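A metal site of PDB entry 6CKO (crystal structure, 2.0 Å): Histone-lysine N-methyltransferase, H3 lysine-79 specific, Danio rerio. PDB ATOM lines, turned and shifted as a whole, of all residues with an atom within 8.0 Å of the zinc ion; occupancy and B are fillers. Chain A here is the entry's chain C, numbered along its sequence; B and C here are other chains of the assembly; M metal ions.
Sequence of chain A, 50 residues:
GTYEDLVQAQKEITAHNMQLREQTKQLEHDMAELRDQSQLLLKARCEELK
OE1 of Glu 33 lies within salt-bridge range of NZ of Lys 66 of chain C.
Within 4 Å of the zinc ion: His 29 of chain A, Glu 33 and Asp 30 of chain B.
The zinc ion is bound by OE2 of Glu 33 (1.9 Å).
The zinc ion is bound by OD2 of Asp 30 of chain B (1.9 Å).
NE2 of His 29 of chain A is bound to the zinc ion, at 2.0 Å.
The zinc ion has three donor atoms within binding distance.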
ATOM      1  N   GLN A  26     -16.437  -1.444   5.691  1.00  0.00           N
ATOM      2  CA  GLN A  26     -15.625  -2.070   4.638  1.00  0.00           C
ATOM      3  C   GLN A  26     -15.919  -3.542   4.551  1.00  0.00           C
ATOM      4  O   GLN A  26     -16.060  -4.086   3.451  1.00  0.00           O
ATOM      5  CB  GLN A  26     -14.115  -1.809   4.877  1.00  0.00           C
ATOM      6  CG  GLN A  26     -13.782  -0.291   4.724  1.00  0.00           C
ATOM      7  CD  GLN A  26     -12.362   0.019   5.209  1.00  0.00           C
ATOM      8  OE1 GLN A  26     -11.808  -0.683   6.055  1.00  0.00           O
ATOM      9  NE2 GLN A  26     -11.771   1.004   4.636  1.00  0.00           N
ATOM     10  N   HIS A  29     -19.178  -4.365   3.021  1.00  0.00           N
ATOM     11  CA  HIS A  29     -19.039  -4.360   1.600  1.00  0.00           C
ATOM     12  C   HIS A  29     -18.291  -5.608   1.084  1.00  0.00           C
ATOM     13  O   HIS A  29     -18.707  -6.210   0.062  1.00  0.00           O
ATOM     14  CB  HIS A  29     -18.361  -3.089   1.026  1.00  0.00           C
ATOM     15  CG  HIS A  29     -18.383  -3.056  -0.469  1.00  0.00           C
ATOM     16  ND1 HIS A  29     -19.532  -2.775  -1.171  1.00  0.00           N
ATOM     17  CD2 HIS A  29     -17.425  -3.340  -1.404  1.00  0.00           C
ATOM     18  CE1 HIS A  29     -19.275  -2.840  -2.478  1.00  0.00           C
ATOM     19  NE2 HIS A  29     -18.010  -3.161  -2.633  1.00  0.00           N
ATOM     20  N   ASP A  30     -17.215  -5.985   1.774  1.00  0.00           N
ATOM     21  CA  ASP A  30     -16.480  -7.190   1.417  1.00  0.00           C
ATOM     22  C   ASP A  30     -17.447  -8.371   1.361  1.00  0.00           C
ATOM     23  O   ASP A  30     -17.349  -9.182   0.422  1.00  0.00           O
ATOM     24  CB  ASP A  30     -15.380  -7.571   2.396  1.00  0.00           C
ATOM     25  CG  ASP A  30     -14.222  -6.606   2.428  1.00  0.00           C
ATOM     26  OD1 ASP A  30     -13.837  -6.002   1.417  1.00  0.00           O
ATOM     27  OD2 ASP A  30     -13.659  -6.487   3.526  1.00  0.00           O
ATOM     28  N   ALA A  32     -20.790  -8.431   0.788  1.00  0.00           N
ATOM     29  CA  ALA A  32     -21.686  -8.321  -0.365  1.00  0.00           C
ATOM     30  C   ALA A  32     -21.004  -8.742  -1.650  1.00  0.00           C
ATOM     31  O   ALA A  32     -21.604  -9.483  -2.450  1.00  0.00           O
ATOM     32  CB  ALA A  32     -22.275  -6.904  -0.481  1.00  0.00           C
ATOM     33  N   GLU A  33     -19.743  -8.352  -1.808  1.00  0.00           N
ATOM     34  CA  GLU A  33     -18.934  -8.768  -2.961  1.00  0.00           C
ATOM     35  C   GLU A  33     -18.744 -10.299  -2.938  1.00  0.00           C
ATOM     36  O   GLU A  33     -18.877 -10.989  -3.955  1.00  0.00           O
ATOM     37  CB  GLU A  33     -17.561  -8.050  -2.964  1.00  0.00           C
ATOM     38  CG  GLU A  33     -17.618  -6.532  -3.338  1.00  0.00           C
ATOM     39  CD  GLU A  33     -17.696  -6.267  -4.834  1.00  0.00           C
ATOM     40  OE1 GLU A  33     -17.615  -7.243  -5.585  1.00  0.00           O
ATOM     41  OE2 GLU A  33     -17.770  -5.083  -5.284  1.00  0.00           O
ATOM     42  N   LEU A  34     -18.398 -10.820  -1.765  1.00  0.00           N
ATOM     43  CA  LEU A  34     -18.128 -12.234  -1.642  1.00  0.00           C
ATOM     44  C   LEU A  34     -19.353 -13.108  -1.912  1.00  0.00           C
ATOM     45  O   LEU A  34     -19.243 -14.096  -2.611  1.00  0.00           O
ATOM     46  CB  LEU A  34     -17.441 -12.576  -0.305  1.00  0.00           C
ATOM     47  CG  LEU A  34     -15.975 -12.118  -0.239  1.00  0.00           C
ATOM     48  CD1 LEU A  34     -15.450 -12.061   1.186  1.00  0.00           C
ATOM     49  CD2 LEU A  34     -15.089 -12.975  -1.124  1.00  0.00           C
ATOM     50  N   GLU B  22     -19.557   7.264  -3.602  1.00  0.00           N
ATOM     51  CA  GLU B  22     -19.461   6.166  -2.626  1.00  0.00           C
ATOM     52  C   GLU B  22     -18.886   4.878  -3.194  1.00  0.00           C
ATOM     53  O   GLU B  22     -18.038   4.229  -2.582  1.00  0.00           O
ATOM     54  CB  GLU B  22     -20.833   5.898  -2.010  1.00  0.00           C
ATOM     55  CG  GLU B  22     -20.750   4.846  -0.912  1.00  0.00           C
ATOM     56  N   GLN B  23     -19.302   4.529  -4.413  1.00  0.00           N
ATOM     57  CA  GLN B  23     -18.808   3.353  -5.063  1.00  0.00           C
ATOM     58  C   GLN B  23     -17.291   3.409  -5.371  1.00  0.00           C
ATOM     59  O   GLN B  23     -16.609   2.383  -5.394  1.00  0.00           O
ATOM     60  CB  GLN B  23     -19.629   3.095  -6.306  1.00  0.00           C
ATOM     61  CG  GLN B  23     -19.348   1.736  -6.837  1.00  0.00           C
ATOM     62  CD  GLN B  23     -20.048   1.362  -8.120  1.00  0.00           C
ATOM     63  OE1 GLN B  23     -20.643   2.177  -8.809  1.00  0.00           O
ATOM     64  NE2 GLN B  23     -19.971   0.066  -8.439  1.00  0.00           N
ATOM     65  N   THR B  24     -16.764   4.616  -5.607  1.00  0.00           N
ATOM     66  CA  THR B  24     -15.348   4.795  -5.799  1.00  0.00           C
ATOM     67  C   THR B  24     -14.581   4.303  -4.553  1.00  0.00           C
ATOM     68  O   THR B  24     -13.583   3.600  -4.661  1.00  0.00           O
ATOM     69  CB  THR B  24     -15.057   6.297  -6.128  1.00  0.00           C
ATOM     70  OG1 THR B  24     -15.578   6.576  -7.414  1.00  0.00           O
ATOM     71  CG2 THR B  24     -13.564   6.587  -6.127  1.00  0.00           C
ATOM     72  N   LYS B  25     -15.041   4.693  -3.384  1.00  0.00           N
ATOM     73  CA  LYS B  25     -14.418   4.297  -2.149  1.00  0.00           C
ATOM     74  C   LYS B  25     -14.518   2.782  -1.946  1.00  0.00           C
ATOM     75  O   LYS B  25     -13.571   2.154  -1.447  1.00  0.00           O
ATOM     76  CB  LYS B  25     -15.063   5.019  -0.964  1.00  0.00           C
ATOM     77  CG  LYS B  25     -14.832   6.531  -0.935  1.00  0.00           C
ATOM     78  CD  LYS B  25     -15.712   7.154   0.132  1.00  0.00           C
ATOM     79  N   GLN B  26     -15.654   2.206  -2.321  1.00  0.00           N
ATOM     80  CA  GLN B  26     -15.856   0.755  -2.155  1.00  0.00           C
ATOM     81  C   GLN B  26     -14.891  -0.007  -3.020  1.00  0.00           C
ATOM     82  O   GLN B  26     -14.293  -0.989  -2.570  1.00  0.00           O
ATOM     83  CB  GLN B  26     -17.316   0.356  -2.459  1.00  0.00           C
ATOM     84  CG  GLN B  26     -18.288   0.966  -1.399  1.00  0.00           C
ATOM     85  CD  GLN B  26     -19.751   0.798  -1.824  1.00  0.00           C
ATOM     86  OE1 GLN B  26     -20.065   0.702  -3.010  1.00  0.00           O
ATOM     87  NE2 GLN B  26     -20.602   0.698  -0.865  1.00  0.00           N
ATOM     88  N   LEU B  27     -14.814   0.419  -4.285  1.00  0.00           N
ATOM     89  CA  LEU B  27     -13.941  -0.185  -5.267  1.00  0.00           C
ATOM     90  C   LEU B  27     -12.447  -0.041  -4.896  1.00  0.00           C
ATOM     91  O   LEU B  27     -11.665  -0.958  -5.132  1.00  0.00           O
ATOM     92  CB  LEU B  27     -14.231   0.375  -6.681  1.00  0.00           C
ATOM     93  CG  LEU B  27     -15.405  -0.146  -7.503  1.00  0.00           C
ATOM     94  CD1 LEU B  27     -15.774   0.825  -8.637  1.00  0.00           C
ATOM     95  CD2 LEU B  27     -15.152  -1.500  -8.089  1.00  0.00           C
ATOM     96  N   GLU B  28     -12.071   1.100  -4.319  1.00  0.00           N
ATOM     97  CA  GLU B  28     -10.723   1.289  -3.786  1.00  0.00           C
ATOM     98  C   GLU B  28     -10.413   0.267  -2.706  1.00  0.00           C
ATOM     99  O   GLU B  28      -9.295  -0.300  -2.677  1.00  0.00           O
ATOM    100  CB  GLU B  28     -10.472   2.713  -3.327  1.00  0.00           C
ATOM    101  CG  GLU B  28     -10.476   3.639  -4.576  1.00  0.00           C
ATOM    102  CD  GLU B  28     -10.483   5.091  -4.256  1.00  0.00           C
ATOM    103  OE1 GLU B  28     -10.781   5.472  -3.112  1.00  0.00           O
ATOM    104  OE2 GLU B  28     -10.154   5.854  -5.153  1.00  0.00           O
ATOM    105  N   HIS B  29     -11.391   0.039  -1.827  1.00  0.00           N
ATOM    106  CA  HIS B  29     -11.228  -0.982  -0.824  1.00  0.00           C
ATOM    107  C   HIS B  29     -11.175  -2.389  -1.455  1.00  0.00           C
ATOM    108  O   HIS B  29     -10.322  -3.225  -1.037  1.00  0.00           O
ATOM    109  CB  HIS B  29     -12.292  -0.953   0.288  1.00  0.00           C
ATOM    110  CG  HIS B  29     -11.989  -1.926   1.382  1.00  0.00           C
ATOM    111  ND1 HIS B  29     -10.988  -1.694   2.312  1.00  0.00           N
ATOM    112  CD2 HIS B  29     -12.489  -3.167   1.668  1.00  0.00           C
ATOM    113  CE1 HIS B  29     -10.921  -2.727   3.143  1.00  0.00           C
ATOM    114  NE2 HIS B  29     -11.831  -3.617   2.789  1.00  0.00           N
ATOM    115  N   ASP B  30     -12.059  -2.651  -2.417  1.00  0.00           N
ATOM    116  CA  ASP B  30     -12.050  -3.928  -3.118  1.00  0.00           C
ATOM    117  C   ASP B  30     -10.651  -4.184  -3.675  1.00  0.00           C
ATOM    118  O   ASP B  30     -10.164  -5.324  -3.567  1.00  0.00           O
ATOM    119  CB  ASP B  30     -13.010  -4.008  -4.294  1.00  0.00           C
ATOM    120  CG  ASP B  30     -14.467  -3.981  -3.903  1.00  0.00           C
ATOM    121  OD1 ASP B  30     -14.873  -4.497  -2.846  1.00  0.00           O
ATOM    122  OD2 ASP B  30     -15.234  -3.447  -4.716  1.00  0.00           O
ATOM    123  N   MET B  31     -10.039  -3.181  -4.300  1.00  0.00           N
ATOM    124  CA  MET B  31      -8.681  -3.321  -4.815  1.00  0.00           C
ATOM    125  C   MET B  31      -7.578  -3.647  -3.802  1.00  0.00           C
ATOM    126  O   MET B  31      -6.674  -4.455  -4.101  1.00  0.00           O
ATOM    127  CB  MET B  31      -8.258  -2.068  -5.604  1.00  0.00           C
ATOM    128  CG  MET B  31      -7.736  -2.424  -6.969  1.00  0.00           C
ATOM    129  SD  MET B  31      -8.987  -3.051  -8.098  1.00  0.00           S
ATOM    130  CE  MET B  31     -10.034  -1.630  -8.253  1.00  0.00           C
ATOM    131  N   LEU B  34      -8.049  -7.233  -2.891  1.00  0.00           N
ATOM    132  CA  LEU B  34      -7.638  -8.088  -3.982  1.00  0.00           C
ATOM    133  C   LEU B  34      -6.127  -8.195  -4.122  1.00  0.00           C
ATOM    134  O   LEU B  34      -5.607  -9.277  -4.313  1.00  0.00           O
ATOM    135  CB  LEU B  34      -8.335  -7.711  -5.304  1.00  0.00           C
ATOM    136  CG  LEU B  34      -9.823  -8.098  -5.340  1.00  0.00           C
ATOM    137  CD1 LEU B  34     -10.587  -7.357  -6.424  1.00  0.00           C
ATOM    138  CD2 LEU B  34     -10.001  -9.600  -5.460  1.00  0.00           C
ATOM    139  N   THR C  63     -13.597  -0.779 -11.939  1.00  0.00           N
ATOM    140  CA  THR C  63     -14.366  -2.005 -12.198  1.00  0.00           C
ATOM    141  C   THR C  63     -13.597  -2.988 -13.028  1.00  0.00           C
ATOM    142  O   THR C  63     -13.514  -4.173 -12.624  1.00  0.00           O
ATOM    143  CB  THR C  63     -15.758  -1.721 -12.761  1.00  0.00           C
ATOM    144  OG1 THR C  63     -16.432  -0.868 -11.824  1.00  0.00           O
ATOM    145  CG2 THR C  63     -16.587  -3.019 -12.973  1.00  0.00           C
ATOM    146  N   LYS C  66     -10.672  -4.466 -10.914  1.00  0.00           N
ATOM    147  CA  LYS C  66     -11.274  -5.381  -9.959  1.00  0.00           C
ATOM    148  C   LYS C  66     -11.578  -6.735 -10.594  1.00  0.00           C
ATOM    149  O   LYS C  66     -11.194  -7.760 -10.062  1.00  0.00           O
ATOM    150  CB  LYS C  66     -12.573  -4.799  -9.328  1.00  0.00           C
ATOM    151  CG  LYS C  66     -13.423  -5.780  -8.499  1.00  0.00           C
ATOM    152  CD  LYS C  66     -14.819  -5.211  -8.143  1.00  0.00           C
ATOM    153  CE  LYS C  66     -15.756  -6.290  -7.727  1.00  0.00           C
ATOM    154  NZ  LYS C  66     -17.190  -5.996  -7.946  1.00  0.00           N
ATOM    155  N   GLN C  70      -9.873 -10.337  -9.752  1.00  0.00           N
ATOM    156  CA  GLN C  70     -10.669 -11.503  -9.322  1.00  0.00           C
ATOM    157  C   GLN C  70     -10.311 -12.700 -10.153  1.00  0.00           C
ATOM    158  O   GLN C  70     -10.148 -13.809  -9.604  1.00  0.00           O
ATOM    159  CB  GLN C  70     -12.194 -11.231  -9.396  1.00  0.00           C
ATOM    160  CG  GLN C  70     -12.611 -10.197  -8.358  1.00  0.00           C
ATOM    161  CD  GLN C  70     -14.069  -9.796  -8.421  1.00  0.00           C
ATOM    162  OE1 GLN C  70     -14.603  -9.527  -9.455  1.00  0.00           O
ATOM    163  NE2 GLN C  70     -14.721  -9.755  -7.283  1.00  0.00           N
HETATM  164 ZN    ZN M   1     -17.148  -3.474  -4.413  1.00  0.00          ZN
